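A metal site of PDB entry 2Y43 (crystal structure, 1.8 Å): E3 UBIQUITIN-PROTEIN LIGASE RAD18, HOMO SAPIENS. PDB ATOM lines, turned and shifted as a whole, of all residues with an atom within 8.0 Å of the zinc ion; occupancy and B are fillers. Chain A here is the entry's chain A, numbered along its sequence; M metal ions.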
ATOM      1  N   ILE A  38     -27.552  -2.839  25.415  1.00  0.00           N
ATOM      2  CA  ILE A  38     -26.805  -3.287  24.225  1.00  0.00           C
ATOM      3  C   ILE A  38     -27.861  -3.466  23.134  1.00  0.00           C
ATOM      4  O   ILE A  38     -28.643  -4.404  23.189  1.00  0.00           O
ATOM      5  CB  ILE A  38     -26.093  -4.632  24.484  1.00  0.00           C
ATOM      6  CG1 ILE A  38     -25.177  -4.546  25.720  1.00  0.00           C
ATOM      7  CG2 ILE A  38     -25.320  -5.062  23.205  1.00  0.00           C
ATOM      8  CD1 ILE A  38     -24.661  -5.939  26.205  1.00  0.00           C
ATOM      9  N   GLN A  40     -27.998  -4.548  20.032  1.00  0.00           N
ATOM     10  CA  GLN A  40     -28.059  -5.736  19.183  1.00  0.00           C
ATOM     11  C   GLN A  40     -28.734  -6.928  19.855  1.00  0.00           C
ATOM     12  O   GLN A  40     -29.177  -7.812  19.165  1.00  0.00           O
ATOM     13  CB  GLN A  40     -26.666  -6.147  18.647  1.00  0.00           C
ATOM     14  CG  GLN A  40     -25.590  -6.288  19.727  1.00  0.00           C
ATOM     15  CD  GLN A  40     -24.759  -5.018  19.889  1.00  0.00           C
ATOM     16  OE1 GLN A  40     -25.316  -3.916  19.991  1.00  0.00           O
ATOM     17  NE2 GLN A  40     -23.442  -5.169  19.920  1.00  0.00           N
ATOM     18  N   CYS A  41     -28.808  -6.946  21.182  1.00  0.00           N
ATOM     19  CA  CYS A  41     -29.375  -8.095  21.887  1.00  0.00           C
ATOM     20  C   CYS A  41     -30.411  -7.728  22.944  1.00  0.00           C
ATOM     21  O   CYS A  41     -31.113  -8.625  23.439  1.00  0.00           O
ATOM     22  CB  CYS A  41     -28.279  -8.948  22.545  1.00  0.00           C
ATOM     23  SG  CYS A  41     -27.279  -8.099  23.813  1.00  0.00           S
ATOM     24  N   SER A  42     -30.472  -6.436  23.295  1.00  0.00           N
ATOM     25  CA  SER A  42     -31.417  -5.879  24.262  1.00  0.00           C
ATOM     26  C   SER A  42     -31.128  -6.208  25.732  1.00  0.00           C
ATOM     27  O   SER A  42     -31.968  -5.983  26.606  1.00  0.00           O
ATOM     28  CB  SER A  42     -32.884  -6.259  23.900  1.00  0.00           C
ATOM     29  OG  SER A  42     -33.793  -5.207  24.289  1.00  0.00           O
ATOM     30  N   HIS A  43     -29.929  -6.706  26.044  1.00  0.00           N
ATOM     31  CA  HIS A  43     -29.593  -6.891  27.443  1.00  0.00           C
ATOM     32  C   HIS A  43     -29.079  -5.570  28.030  1.00  0.00           C
ATOM     33  O   HIS A  43     -28.572  -4.713  27.296  1.00  0.00           O
ATOM     34  CB  HIS A  43     -28.604  -8.052  27.632  1.00  0.00           C
ATOM     35  CG  HIS A  43     -29.194  -9.372  27.231  1.00  0.00           C
ATOM     36  ND1 HIS A  43     -28.598 -10.199  26.300  1.00  0.00           N
ATOM     37  CD2 HIS A  43     -30.333  -9.992  27.608  1.00  0.00           C
ATOM     38  CE1 HIS A  43     -29.359 -11.267  26.114  1.00  0.00           C
ATOM     39  NE2 HIS A  43     -30.416 -11.171  26.892  1.00  0.00           N
ATOM     40  N   ASN A  44     -29.238  -5.415  29.343  1.00  0.00           N
ATOM     41  CA  ASN A  44     -28.953  -4.185  30.057  1.00  0.00           C
ATOM     42  C   ASN A  44     -28.021  -4.431  31.247  1.00  0.00           C
ATOM     43  O   ASN A  44     -28.118  -5.472  31.923  1.00  0.00           O
ATOM     44  CB  ASN A  44     -30.241  -3.587  30.620  1.00  0.00           C
ATOM     45  CG  ASN A  44     -31.253  -3.273  29.541  1.00  0.00           C
ATOM     46  OD1 ASN A  44     -31.141  -2.260  28.864  1.00  0.00           O
ATOM     47  ND2 ASN A  44     -32.235  -4.132  29.386  1.00  0.00           N
ATOM     48  N   TYR A  45     -27.154  -3.456  31.503  1.00  0.00           N
ATOM     49  CA  TYR A  45     -26.176  -3.482  32.613  1.00  0.00           C
ATOM     50  C   TYR A  45     -25.938  -2.060  33.097  1.00  0.00           C
ATOM     51  O   TYR A  45     -26.163  -1.121  32.341  1.00  0.00           O
ATOM     52  CB  TYR A  45     -24.801  -4.033  32.162  1.00  0.00           C
ATOM     53  CG  TYR A  45     -24.954  -5.405  31.578  1.00  0.00           C
ATOM     54  CD1 TYR A  45     -25.019  -6.518  32.420  1.00  0.00           C
ATOM     55  CD2 TYR A  45     -25.117  -5.574  30.220  1.00  0.00           C
ATOM     56  CE1 TYR A  45     -25.221  -7.792  31.892  1.00  0.00           C
ATOM     57  CE2 TYR A  45     -25.324  -6.854  29.679  1.00  0.00           C
ATOM     58  CZ  TYR A  45     -25.375  -7.941  30.514  1.00  0.00           C
ATOM     59  OH  TYR A  45     -25.576  -9.163  29.970  1.00  0.00           O
ATOM     60  N   GLN A  59     -17.874  -8.869  24.577  1.00  0.00           N
ATOM     61  CA  GLN A  59     -19.082  -9.677  24.380  1.00  0.00           C
ATOM     62  C   GLN A  59     -20.121  -9.300  25.401  1.00  0.00           C
ATOM     63  O   GLN A  59     -19.782  -8.795  26.472  1.00  0.00           O
ATOM     64  CB  GLN A  59     -18.776 -11.157  24.603  1.00  0.00           C
ATOM     65  CG  GLN A  59     -17.974 -11.847  23.541  1.00  0.00           C
ATOM     66  CD  GLN A  59     -17.477 -13.210  24.003  1.00  0.00           C
ATOM     67  OE1 GLN A  59     -18.170 -13.920  24.736  1.00  0.00           O
ATOM     68  NE2 GLN A  59     -16.262 -13.558  23.589  1.00  0.00           N
ATOM     69  N   CYS A  60     -21.384  -9.589  25.100  1.00  0.00           N
ATOM     70  CA  CYS A  60     -22.444  -9.510  26.089  1.00  0.00           C
ATOM     71  C   CYS A  60     -22.245 -10.647  27.087  1.00  0.00           C
ATOM     72  O   CYS A  60     -22.129 -11.798  26.679  1.00  0.00           O
ATOM     73  CB  CYS A  60     -23.816  -9.633  25.445  1.00  0.00           C
ATOM     74  SG  CYS A  60     -25.189  -9.688  26.648  1.00  0.00           S
ATOM     75  N   PRO A  61     -22.202 -10.329  28.397  1.00  0.00           N
ATOM     76  CA  PRO A  61     -22.044 -11.342  29.451  1.00  0.00           C
ATOM     77  C   PRO A  61     -23.134 -12.433  29.459  1.00  0.00           C
ATOM     78  O   PRO A  61     -22.877 -13.563  29.908  1.00  0.00           O
ATOM     79  CB  PRO A  61     -22.131 -10.522  30.746  1.00  0.00           C
ATOM     80  CG  PRO A  61     -21.856  -9.146  30.380  1.00  0.00           C
ATOM     81  CD  PRO A  61     -22.183  -8.953  28.918  1.00  0.00           C
ATOM     82  N   THR A  62     -24.322 -12.096  28.970  1.00  0.00           N
ATOM     83  CA  THR A  62     -25.471 -13.025  29.001  1.00  0.00           C
ATOM     84  C   THR A  62     -25.544 -13.881  27.736  1.00  0.00           C
ATOM     85  O   THR A  62     -25.628 -15.115  27.820  1.00  0.00           O
ATOM     86  CB  THR A  62     -26.798 -12.252  29.186  1.00  0.00           C
ATOM     87  OG1 THR A  62     -26.724 -11.499  30.407  1.00  0.00           O
ATOM     88  CG2 THR A  62     -27.993 -13.206  29.275  1.00  0.00           C
ATOM     89  N   CYS A  63     -25.468 -13.251  26.576  1.00  0.00           N
ATOM     90  CA  CYS A  63     -25.707 -13.961  25.319  1.00  0.00           C
ATOM     91  C   CYS A  63     -24.473 -14.156  24.411  1.00  0.00           C
ATOM     92  O   CYS A  63     -24.547 -14.868  23.406  1.00  0.00           O
ATOM     93  CB  CYS A  63     -26.859 -13.307  24.558  1.00  0.00           C
ATOM     94  SG  CYS A  63     -26.430 -11.767  23.736  1.00  0.00           S
ATOM     95  N   CYS A  64     -23.359 -13.510  24.759  1.00  0.00           N
ATOM     96  CA  CYS A  64     -22.030 -13.707  24.127  1.00  0.00           C
ATOM     97  C   CYS A  64     -21.859 -13.113  22.716  1.00  0.00           C
ATOM     98  O   CYS A  64     -20.837 -13.338  22.079  1.00  0.00           O
ATOM     99  CB  CYS A  64     -21.591 -15.171  24.143  1.00  0.00           C
ATOM    100  SG  CYS A  64     -21.673 -15.936  25.801  1.00  0.00           S
ATOM    101  N   VAL A  65     -22.859 -12.377  22.248  1.00  0.00           N
ATOM    102  CA  VAL A  65     -22.725 -11.650  20.993  1.00  0.00           C
ATOM    103  C   VAL A  65     -21.602 -10.624  21.172  1.00  0.00           C
ATOM    104  O   VAL A  65     -21.375 -10.143  22.283  1.00  0.00           O
ATOM    105  CB  VAL A  65     -24.083 -10.977  20.545  1.00  0.00           C
ATOM    106  CG1 VAL A  65     -24.416  -9.757  21.376  1.00  0.00           C
ATOM    107  CG2 VAL A  65     -24.056 -10.607  19.071  1.00  0.00           C
ATOM    108  N   THR A  66     -20.905 -10.287  20.084  1.00  0.00           N
ATOM    109  CA  THR A  66     -19.847  -9.278  20.147  1.00  0.00           C
ATOM    110  C   THR A  66     -20.439  -7.897  20.445  1.00  0.00           C
ATOM    111  O   THR A  66     -21.413  -7.454  19.822  1.00  0.00           O
ATOM    112  CB  THR A  66     -18.998  -9.248  18.874  1.00  0.00           C
ATOM    113  OG1 THR A  66     -18.469 -10.558  18.638  1.00  0.00           O
ATOM    114  CG2 THR A  66     -17.794  -8.256  19.016  1.00  0.00           C
ATOM    115  N   VAL A  67     -19.811  -7.218  21.397  1.00  0.00           N
ATOM    116  CA  VAL A  67     -20.213  -5.870  21.808  1.00  0.00           C
ATOM    117  C   VAL A  67     -18.960  -5.037  22.100  1.00  0.00           C
ATOM    118  O   VAL A  67     -17.979  -5.525  22.676  1.00  0.00           O
ATOM    119  CB  VAL A  67     -21.064  -5.924  23.116  1.00  0.00           C
ATOM    120  CG1 VAL A  67     -21.525  -4.505  23.547  1.00  0.00           C
ATOM    121  CG2 VAL A  67     -22.234  -6.899  22.987  1.00  0.00           C
HETATM  122 ZN    ZN M   1     -26.879  -9.951  25.145  1.00  0.00          ZN
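The side-chain sulfur of Cys 60 lies close to the backbone NH of Thr 62, 3.5 Å away.
The side-chain hydroxyl (OH) of Tyr 45 lies close to the side-chain sulfur (SG) of Cys 60, 3.4 Å away.
O of His 43 lies within hydrogen-bond range of N of Ile 38 (2.8 Å).
The backbone NH (N) of Cys 60 lies within hydrogen-bond range of the backbone carbonyl oxygen (O) of Val 65 (2.9 Å).
Four residues have an atom within 4 Å of the zinc ion: Cys 41, His 43, Cys 60 and Cys 63.
The nearest printed residue that does not touch the zinc ion is Val 65 (4.5 Å).
The zinc ion is bound by a ring nitrogen (ND1) of His 43, the side-chain sulfur (SG) of Cys 60, the side-chain sulfur (SG) of Cys 41 and the side-chain sulfur (SG) of Cys 63.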
